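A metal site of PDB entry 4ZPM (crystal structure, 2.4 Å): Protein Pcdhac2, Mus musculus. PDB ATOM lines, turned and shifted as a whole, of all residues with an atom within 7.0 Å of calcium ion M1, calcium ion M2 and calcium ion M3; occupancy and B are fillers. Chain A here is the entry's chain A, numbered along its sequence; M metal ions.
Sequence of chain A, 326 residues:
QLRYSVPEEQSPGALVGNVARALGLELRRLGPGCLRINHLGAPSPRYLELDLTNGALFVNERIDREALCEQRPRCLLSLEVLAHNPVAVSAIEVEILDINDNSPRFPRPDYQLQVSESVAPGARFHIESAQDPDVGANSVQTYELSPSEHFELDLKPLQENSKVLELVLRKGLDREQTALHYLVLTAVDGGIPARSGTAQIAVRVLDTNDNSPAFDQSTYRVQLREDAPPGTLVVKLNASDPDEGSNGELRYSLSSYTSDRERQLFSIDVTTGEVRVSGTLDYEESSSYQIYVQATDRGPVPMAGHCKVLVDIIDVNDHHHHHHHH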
ATOM      1  N   GLU A 117      -7.532 -20.505   0.124  1.00  0.00           N
ATOM      2  CA  GLU A 117      -7.585 -19.407  -0.829  1.00  0.00           C
ATOM      3  C   GLU A 117      -6.492 -18.368  -0.581  1.00  0.00           C
ATOM      4  O   GLU A 117      -6.080 -17.654  -1.489  1.00  0.00           O
ATOM      5  CB  GLU A 117      -8.963 -18.744  -0.752  1.00  0.00           C
ATOM      6  CG  GLU A 117      -9.308 -17.833  -1.884  1.00  0.00           C
ATOM      7  CD  GLU A 117     -10.616 -17.120  -1.655  1.00  0.00           C
ATOM      8  OE1 GLU A 117     -11.272 -17.411  -0.620  1.00  0.00           O
ATOM      9  OE2 GLU A 117     -10.997 -16.279  -2.482  1.00  0.00           O
ATOM     10  N   LEU A 173      -5.551 -18.501  -6.027  1.00  0.00           N
ATOM     11  CA  LEU A 173      -6.864 -19.144  -6.030  1.00  0.00           C
ATOM     12  C   LEU A 173      -7.923 -18.184  -5.519  1.00  0.00           C
ATOM     13  O   LEU A 173      -7.645 -17.308  -4.692  1.00  0.00           O
ATOM     14  CB  LEU A 173      -6.844 -20.408  -5.174  1.00  0.00           C
ATOM     15  CG  LEU A 173      -5.894 -21.528  -5.627  1.00  0.00           C
ATOM     16  CD1 LEU A 173      -5.978 -22.709  -4.668  1.00  0.00           C
ATOM     17  CD2 LEU A 173      -6.212 -21.966  -7.049  1.00  0.00           C
ATOM     18  N   ASP A 174      -9.138 -18.329  -6.024  1.00  0.00           N
ATOM     19  CA  ASP A 174     -10.258 -17.509  -5.580  1.00  0.00           C
ATOM     20  C   ASP A 174     -11.525 -18.346  -5.506  1.00  0.00           C
ATOM     21  O   ASP A 174     -12.145 -18.634  -6.525  1.00  0.00           O
ATOM     22  CB  ASP A 174     -10.462 -16.316  -6.516  1.00  0.00           C
ATOM     23  CG  ASP A 174     -11.579 -15.391  -6.077  1.00  0.00           C
ATOM     24  OD1 ASP A 174     -12.051 -15.518  -4.920  1.00  0.00           O
ATOM     25  OD2 ASP A 174     -11.997 -14.536  -6.891  1.00  0.00           O
ATOM     26  N   ARG A 175     -11.898 -18.741  -4.289  1.00  0.00           N
ATOM     27  CA  ARG A 175     -13.038 -19.626  -4.080  1.00  0.00           C
ATOM     28  C   ARG A 175     -14.346 -19.003  -4.592  1.00  0.00           C
ATOM     29  O   ARG A 175     -15.241 -19.720  -5.058  1.00  0.00           O
ATOM     30  CB  ARG A 175     -13.190 -19.976  -2.598  1.00  0.00           C
ATOM     31  CG  ARG A 175     -14.329 -20.926  -2.320  1.00  0.00           C
ATOM     32  CD  ARG A 175     -14.871 -20.764  -0.917  1.00  0.00           C
ATOM     33  NE  ARG A 175     -15.602 -19.509  -0.783  1.00  0.00           N
ATOM     34  CZ  ARG A 175     -16.855 -19.317  -1.188  1.00  0.00           C
ATOM     35  NH1 ARG A 175     -17.521 -20.307  -1.764  1.00  0.00           N
ATOM     36  NH2 ARG A 175     -17.435 -18.138  -1.011  1.00  0.00           N
ATOM     37  N   GLU A 176     -14.453 -17.688  -4.493  1.00  0.00           N
ATOM     38  CA  GLU A 176     -15.644 -16.979  -4.965  1.00  0.00           C
ATOM     39  C   GLU A 176     -15.759 -17.074  -6.483  1.00  0.00           C
ATOM     40  O   GLU A 176     -16.863 -17.059  -7.029  1.00  0.00           O
ATOM     41  CB  GLU A 176     -15.604 -15.519  -4.520  1.00  0.00           C
ATOM     42  CG  GLU A 176     -15.940 -15.348  -3.055  1.00  0.00           C
ATOM     43  CD  GLU A 176     -14.763 -15.637  -2.145  1.00  0.00           C
ATOM     44  OE1 GLU A 176     -14.978 -16.195  -1.053  1.00  0.00           O
ATOM     45  OE2 GLU A 176     -13.617 -15.322  -2.528  1.00  0.00           O
ATOM     46  N   GLN A 177     -14.616 -17.174  -7.148  1.00  0.00           N
ATOM     47  CA  GLN A 177     -14.577 -17.414  -8.585  1.00  0.00           C
ATOM     48  C   GLN A 177     -14.788 -18.907  -8.876  1.00  0.00           C
ATOM     49  O   GLN A 177     -15.689 -19.273  -9.623  1.00  0.00           O
ATOM     50  CB  GLN A 177     -13.247 -16.937  -9.174  1.00  0.00           C
ATOM     51  CG  GLN A 177     -13.223 -16.857 -10.685  1.00  0.00           C
ATOM     52  CD  GLN A 177     -12.317 -15.756 -11.189  1.00  0.00           C
ATOM     53  OE1 GLN A 177     -11.746 -14.985 -10.411  1.00  0.00           O
ATOM     54  NE2 GLN A 177     -12.164 -15.677 -12.512  1.00  0.00           N
ATOM     55  N   LEU A 206     -10.419 -23.659  -0.076  1.00  0.00           N
ATOM     56  CA  LEU A 206     -11.071 -23.343   1.185  1.00  0.00           C
ATOM     57  C   LEU A 206     -11.276 -21.846   1.305  1.00  0.00           C
ATOM     58  O   LEU A 206     -10.467 -21.063   0.819  1.00  0.00           O
ATOM     59  CB  LEU A 206     -10.237 -23.867   2.358  1.00  0.00           C
ATOM     60  CG  LEU A 206      -9.885 -25.353   2.330  1.00  0.00           C
ATOM     61  CD1 LEU A 206      -9.065 -25.741   3.554  1.00  0.00           C
ATOM     62  CD2 LEU A 206     -11.143 -26.210   2.231  1.00  0.00           C
ATOM     63  N   ASP A 207     -12.369 -21.448   1.960  1.00  0.00           N
ATOM     64  CA  ASP A 207     -12.724 -20.040   2.058  1.00  0.00           C
ATOM     65  C   ASP A 207     -11.888 -19.287   3.087  1.00  0.00           C
ATOM     66  O   ASP A 207     -11.667 -19.782   4.195  1.00  0.00           O
ATOM     67  CB  ASP A 207     -14.211 -19.873   2.405  1.00  0.00           C
ATOM     68  CG  ASP A 207     -14.655 -18.429   2.402  1.00  0.00           C
ATOM     69  OD1 ASP A 207     -14.351 -17.709   1.432  1.00  0.00           O
ATOM     70  OD2 ASP A 207     -15.302 -18.000   3.383  1.00  0.00           O
ATOM     71  N   THR A 208     -11.408 -18.110   2.714  1.00  0.00           N
ATOM     72  CA  THR A 208     -10.861 -17.169   3.681  1.00  0.00           C
ATOM     73  C   THR A 208     -11.749 -15.937   3.691  1.00  0.00           C
ATOM     74  O   THR A 208     -12.473 -15.669   2.728  1.00  0.00           O
ATOM     75  CB  THR A 208      -9.413 -16.768   3.362  1.00  0.00           C
ATOM     76  OG1 THR A 208      -9.403 -15.901   2.218  1.00  0.00           O
ATOM     77  CG2 THR A 208      -8.561 -17.994   3.077  1.00  0.00           C
ATOM     78  N   ASN A 209     -11.703 -15.179   4.780  1.00  0.00           N
ATOM     79  CA  ASN A 209     -12.494 -13.956   4.872  1.00  0.00           C
ATOM     80  C   ASN A 209     -11.782 -12.807   4.181  1.00  0.00           C
ATOM     81  O   ASN A 209     -11.296 -11.882   4.836  1.00  0.00           O
ATOM     82  CB  ASN A 209     -12.771 -13.610   6.341  1.00  0.00           C
ATOM     83  CG  ASN A 209     -13.922 -12.649   6.499  1.00  0.00           C
ATOM     84  OD1 ASN A 209     -14.407 -12.079   5.528  1.00  0.00           O
ATOM     85  ND2 ASN A 209     -14.360 -12.452   7.743  1.00  0.00           N
ATOM     86  N   ASP A 210     -11.732 -12.856   2.857  1.00  0.00           N
ATOM     87  CA  ASP A 210     -10.960 -11.892   2.082  1.00  0.00           C
ATOM     88  C   ASP A 210     -11.848 -10.871   1.361  1.00  0.00           C
ATOM     89  O   ASP A 210     -11.366 -10.080   0.553  1.00  0.00           O
ATOM     90  CB  ASP A 210     -10.068 -12.604   1.071  1.00  0.00           C
ATOM     91  CG  ASP A 210     -10.852 -13.449   0.084  1.00  0.00           C
ATOM     92  OD1 ASP A 210     -12.030 -13.764   0.367  1.00  0.00           O
ATOM     93  OD2 ASP A 210     -10.290 -13.805  -0.979  1.00  0.00           O
ATOM     94  N   ASN A 211     -13.141 -10.884   1.688  1.00  0.00           N
ATOM     95  CA  ASN A 211     -14.076  -9.903   1.150  1.00  0.00           C
ATOM     96  C   ASN A 211     -14.779  -9.159   2.274  1.00  0.00           C
ATOM     97  O   ASN A 211     -15.281  -9.777   3.217  1.00  0.00           O
ATOM     98  CB  ASN A 211     -15.109 -10.576   0.240  1.00  0.00           C
ATOM     99  CG  ASN A 211     -14.538 -10.980  -1.107  1.00  0.00           C
ATOM    100  OD1 ASN A 211     -14.561 -10.197  -2.059  1.00  0.00           O
ATOM    101  ND2 ASN A 211     -14.030 -12.195  -1.189  1.00  0.00           N
ATOM    102  N   SER A 212     -14.820  -7.841   2.174  1.00  0.00           N
ATOM    103  CA  SER A 212     -15.540  -7.030   3.144  1.00  0.00           C
ATOM    104  C   SER A 212     -16.927  -6.696   2.613  1.00  0.00           C
ATOM    105  O   SER A 212     -17.105  -6.563   1.403  1.00  0.00           O
ATOM    106  CB  SER A 212     -14.750  -5.752   3.462  1.00  0.00           C
ATOM    107  OG  SER A 212     -14.274  -5.136   2.289  1.00  0.00           O
ATOM    108  N   PRO A 213     -17.913  -6.583   3.514  1.00  0.00           N
ATOM    109  CA  PRO A 213     -19.292  -6.235   3.164  1.00  0.00           C
ATOM    110  C   PRO A 213     -19.368  -4.980   2.317  1.00  0.00           C
ATOM    111  O   PRO A 213     -18.555  -4.082   2.490  1.00  0.00           O
ATOM    112  CB  PRO A 213     -19.955  -6.008   4.525  1.00  0.00           C
ATOM    113  CG  PRO A 213     -19.161  -6.846   5.465  1.00  0.00           C
ATOM    114  CD  PRO A 213     -17.749  -6.812   4.965  1.00  0.00           C
ATOM    115  N   ASP A 241     -22.042  -9.939   0.930  1.00  0.00           N
ATOM    116  CA  ASP A 241     -20.707 -10.474   1.144  1.00  0.00           C
ATOM    117  C   ASP A 241     -20.558 -11.834   0.462  1.00  0.00           C
ATOM    118  O   ASP A 241     -21.197 -12.806   0.873  1.00  0.00           O
ATOM    119  CB  ASP A 241     -20.413 -10.597   2.644  1.00  0.00           C
ATOM    120  CG  ASP A 241     -18.928 -10.731   2.932  1.00  0.00           C
ATOM    121  OD1 ASP A 241     -18.379 -11.844   2.768  1.00  0.00           O
ATOM    122  OD2 ASP A 241     -18.307  -9.732   3.347  1.00  0.00           O
ATOM    123  N   PRO A 242     -19.699 -11.922  -0.562  1.00  0.00           N
ATOM    124  CA  PRO A 242     -19.568 -13.117  -1.397  1.00  0.00           C
ATOM    125  C   PRO A 242     -18.847 -14.291  -0.730  1.00  0.00           C
ATOM    126  O   PRO A 242     -18.820 -15.374  -1.304  1.00  0.00           O
ATOM    127  CB  PRO A 242     -18.766 -12.618  -2.601  1.00  0.00           C
ATOM    128  CG  PRO A 242     -17.955 -11.488  -2.055  1.00  0.00           C
ATOM    129  CD  PRO A 242     -18.819 -10.831  -1.020  1.00  0.00           C
ATOM    130  N   ASP A 243     -18.284 -14.085   0.462  1.00  0.00           N
ATOM    131  CA  ASP A 243     -17.575 -15.162   1.150  1.00  0.00           C
ATOM    132  C   ASP A 243     -18.547 -16.247   1.631  1.00  0.00           C
ATOM    133  O   ASP A 243     -19.757 -16.103   1.505  1.00  0.00           O
ATOM    134  CB  ASP A 243     -16.780 -14.613   2.330  1.00  0.00           C
ATOM    135  CG  ASP A 243     -15.586 -13.783   1.882  1.00  0.00           C
ATOM    136  OD1 ASP A 243     -15.154 -13.944   0.722  1.00  0.00           O
ATOM    137  OD2 ASP A 243     -15.076 -12.973   2.689  1.00  0.00           O
ATOM    138  N   GLU A 244     -17.993 -17.326   2.182  1.00  0.00           N
ATOM    139  CA  GLU A 244     -18.782 -18.504   2.494  1.00  0.00           C
ATOM    140  C   GLU A 244     -19.141 -18.618   3.970  1.00  0.00           C
ATOM    141  O   GLU A 244     -18.304 -18.380   4.850  1.00  0.00           O
ATOM    142  CB  GLU A 244     -18.023 -19.763   2.067  1.00  0.00           C
ATOM    143  CG  GLU A 244     -18.680 -21.076   2.463  1.00  0.00           C
ATOM    144  CD  GLU A 244     -17.861 -22.289   2.044  1.00  0.00           C
ATOM    145  OE1 GLU A 244     -16.656 -22.345   2.383  1.00  0.00           O
ATOM    146  OE2 GLU A 244     -18.422 -23.179   1.374  1.00  0.00           O
ATOM    147  N   SER A 246     -20.144 -18.234   7.660  1.00  0.00           N
ATOM    148  CA  SER A 246     -19.998 -17.201   8.671  1.00  0.00           C
ATOM    149  C   SER A 246     -19.230 -15.988   8.147  1.00  0.00           C
ATOM    150  O   SER A 246     -19.445 -14.872   8.603  1.00  0.00           O
ATOM    151  CB  SER A 246     -19.306 -17.767   9.910  1.00  0.00           C
ATOM    152  OG  SER A 246     -19.062 -16.758  10.874  1.00  0.00           O
ATOM    153  N   ASN A 247     -18.333 -16.230   7.196  1.00  0.00           N
ATOM    154  CA  ASN A 247     -17.533 -15.154   6.605  1.00  0.00           C
ATOM    155  C   ASN A 247     -18.336 -14.211   5.709  1.00  0.00           C
ATOM    156  O   ASN A 247     -17.896 -13.098   5.419  1.00  0.00           O
ATOM    157  CB  ASN A 247     -16.376 -15.742   5.806  1.00  0.00           C
ATOM    158  CG  ASN A 247     -15.422 -16.523   6.678  1.00  0.00           C
ATOM    159  OD1 ASN A 247     -14.763 -15.962   7.554  1.00  0.00           O
ATOM    160  ND2 ASN A 247     -15.334 -17.831   6.436  1.00  0.00           N
ATOM    161  N   GLY A 248     -19.498 -14.669   5.254  1.00  0.00           N
ATOM    162  CA  GLY A 248     -20.354 -13.840   4.406  1.00  0.00           C
ATOM    163  C   GLY A 248     -21.646 -13.426   5.098  1.00  0.00           C
ATOM    164  O   GLY A 248     -22.565 -12.926   4.450  1.00  0.00           O
ATOM    165  N   GLU A 249     -21.698 -13.596   6.413  1.00  0.00           N
ATOM    166  CA  GLU A 249     -22.909 -13.300   7.164  1.00  0.00           C
ATOM    167  C   GLU A 249     -22.784 -11.923   7.803  1.00  0.00           C
ATOM    168  O   GLU A 249     -21.803 -11.628   8.481  1.00  0.00           O
ATOM    169  CB  GLU A 249     -23.169 -14.373   8.220  1.00  0.00           C
ATOM    170  CG  GLU A 249     -24.142 -15.446   7.756  1.00  0.00           C
ATOM    171  CD  GLU A 249     -25.182 -15.781   8.801  1.00  0.00           C
ATOM    172  OE1 GLU A 249     -24.887 -15.656  10.005  1.00  0.00           O
ATOM    173  OE2 GLU A 249     -26.315 -16.163   8.412  1.00  0.00           O
ATOM    174  N   LEU A 250     -23.799 -11.093   7.577  1.00  0.00           N
ATOM    175  CA  LEU A 250     -23.726  -9.682   7.920  1.00  0.00           C
ATOM    176  C   LEU A 250     -24.606  -9.291   9.106  1.00  0.00           C
ATOM    177  O   LEU A 250     -25.690  -9.835   9.298  1.00  0.00           O
ATOM    178  CB  LEU A 250     -24.097  -8.834   6.704  1.00  0.00           C
ATOM    179  CG  LEU A 250     -23.330  -9.202   5.434  1.00  0.00           C
ATOM    180  CD1 LEU A 250     -23.673  -8.270   4.290  1.00  0.00           C
ATOM    181  CD2 LEU A 250     -21.834  -9.204   5.698  1.00  0.00           C
ATOM    182  N   ASP A 297     -18.784  -8.489   9.038  1.00  0.00           N
ATOM    183  CA  ASP A 297     -18.694  -9.951   8.916  1.00  0.00           C
ATOM    184  C   ASP A 297     -18.866 -10.650  10.244  1.00  0.00           C
ATOM    185  O   ASP A 297     -18.759 -10.030  11.303  1.00  0.00           O
ATOM    186  CB  ASP A 297     -17.342 -10.360   8.320  1.00  0.00           C
ATOM    187  CG  ASP A 297     -17.261 -10.111   6.837  1.00  0.00           C
ATOM    188  OD1 ASP A 297     -18.326  -9.933   6.210  1.00  0.00           O
ATOM    189  OD2 ASP A 297     -16.138 -10.075   6.306  1.00  0.00           O
ATOM    190  N   ARG A 298     -19.126 -11.946  10.188  1.00  0.00           N
ATOM    191  CA  ARG A 298     -19.066 -12.808  11.361  1.00  0.00           C
ATOM    192  C   ARG A 298     -17.857 -13.742  11.269  1.00  0.00           C
ATOM    193  O   ARG A 298     -17.800 -14.764  11.940  1.00  0.00           O
ATOM    194  CB  ARG A 298     -20.352 -13.619  11.515  1.00  0.00           C
ATOM    195  CG  ARG A 298     -21.530 -12.832  12.051  1.00  0.00           C
ATOM    196  CD  ARG A 298     -22.756 -13.725  12.216  1.00  0.00           C
ATOM    197  N   GLY A 299     -16.896 -13.374  10.427  1.00  0.00           N
ATOM    198  CA  GLY A 299     -15.678 -14.148  10.289  1.00  0.00           C
ATOM    199  C   GLY A 299     -14.744 -13.990  11.478  1.00  0.00           C
ATOM    200  O   GLY A 299     -14.998 -13.177  12.364  1.00  0.00           O
ATOM    201  N   VAL A 301     -11.683 -12.747  11.639  1.00  0.00           N
ATOM    202  CA  VAL A 301     -11.341 -11.327  11.618  1.00  0.00           C
ATOM    203  C   VAL A 301     -12.463 -10.580  10.917  1.00  0.00           C
ATOM    204  O   VAL A 301     -12.513 -10.541   9.688  1.00  0.00           O
ATOM    205  CB  VAL A 301     -10.007 -11.063  10.895  1.00  0.00           C
ATOM    206  CG1 VAL A 301      -9.687  -9.580  10.890  1.00  0.00           C
ATOM    207  CG2 VAL A 301      -8.886 -11.873  11.531  1.00  0.00           C
ATOM    208  N   MET A 303     -14.807  -8.152   9.008  1.00  0.00           N
ATOM    209  CA  MET A 303     -14.519  -7.131   8.022  1.00  0.00           C
ATOM    210  C   MET A 303     -15.767  -6.279   7.855  1.00  0.00           C
ATOM    211  O   MET A 303     -16.875  -6.777   8.035  1.00  0.00           O
ATOM    212  CB  MET A 303     -14.122  -7.749   6.685  1.00  0.00           C
ATOM    213  CG  MET A 303     -12.898  -8.651   6.749  1.00  0.00           C
ATOM    214  SD  MET A 303     -11.349  -7.729   6.707  1.00  0.00           S
ATOM    215  CE  MET A 303     -10.179  -9.030   7.115  1.00  0.00           C
HETATM  216 CA    CA M   1     -16.486 -11.447   4.293  1.00  0.00          CA
HETATM  217 CA    CA M   2     -13.306 -15.767   0.489  1.00  0.00          CA
HETATM  218 CA    CA M   3     -11.305 -14.121  -3.055  1.00  0.00          CA
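The nearest printed residue that does not touch calcium ion M2 is Asn 211 (4.01 Å).
N of Glu 117 sits at hydrogen-bond distance from O of Leu 206.
OE2 of Glu 176 sits close to ND2 of Asn 211, 3.4 Å away.
The guanidinium group (NH2) of Arg 175 lies close to the side-chain carboxylate (OE1) of Glu 176 (3.1 Å).
The side-chain amide nitrogen (ND2) of Asn 211 lies close to the side-chain carboxylate (OD1) of Asp 210 (3.0 Å).
OD1 of Asp 207 lies close to NE of Arg 175 (3.1 Å).
The side-chain carboxylate (OD2) of Asp 207 is in hydrogen-bond range of the backbone NH (N) of Glu 244 (3.0 Å).
The backbone carbonyl oxygen of Met 303 is in hydrogen-bond range of the backbone NH of Asp 297, 2.8 Å away.
ND2 of Asn 209 is in hydrogen-bond range of O of Val 301.
OE2 of Glu 117 binds calcium ion M3 (2.3 Å).
Calcium ion M3 is bound by OD2 of Asp 210, at 2.3 Å.
OD1 of Asp 174 binds calcium ion M3, 2.4 Å away.
Calcium ion M3 is bound by the side-chain carboxylate (OE2) of Glu 176 (2.7 Å).
Calcium ion M1 is bound by O of Asn 211 (2.3 Å), O of Asn 247 (2.4 Å), OD2 of Asp 297 (2.5 Å), OD1 of Asp 241 (2.5 Å), OD1 of Asn 209 (2.5 Å), OD2 of Asp 243 (2.6 Å) and OD2 of Asp 241 (2.7 Å).
Slightly farther from calcium ion M1 lies OD1 of Asp 297 (3.1 Å).
Five residues have an atom within 4 Å of calcium ion M3: Glu 117, Asp 174, Glu 176, Asp 210 and Asn 211.
Calcium ion M2 is bound by the side-chain carboxylate (OE1) of Glu 176, the side-chain carboxylate (OD1) of Asp 210, the backbone carbonyl oxygen (O) of Thr 208, the side-chain carboxylate (OD1) of Asp 207, the side-chain carboxylate (OD1) of Asp 243 and the side-chain carboxylate (OE1) of Glu 117.
Slightly farther from calcium ion M2 lies OE2 of Glu 176 (3.1 Å).
Within 4 Å of calcium ion M1: Asn 209, Asn 211, Asp 241, Asp 243, Asn 247 and Asp 297.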
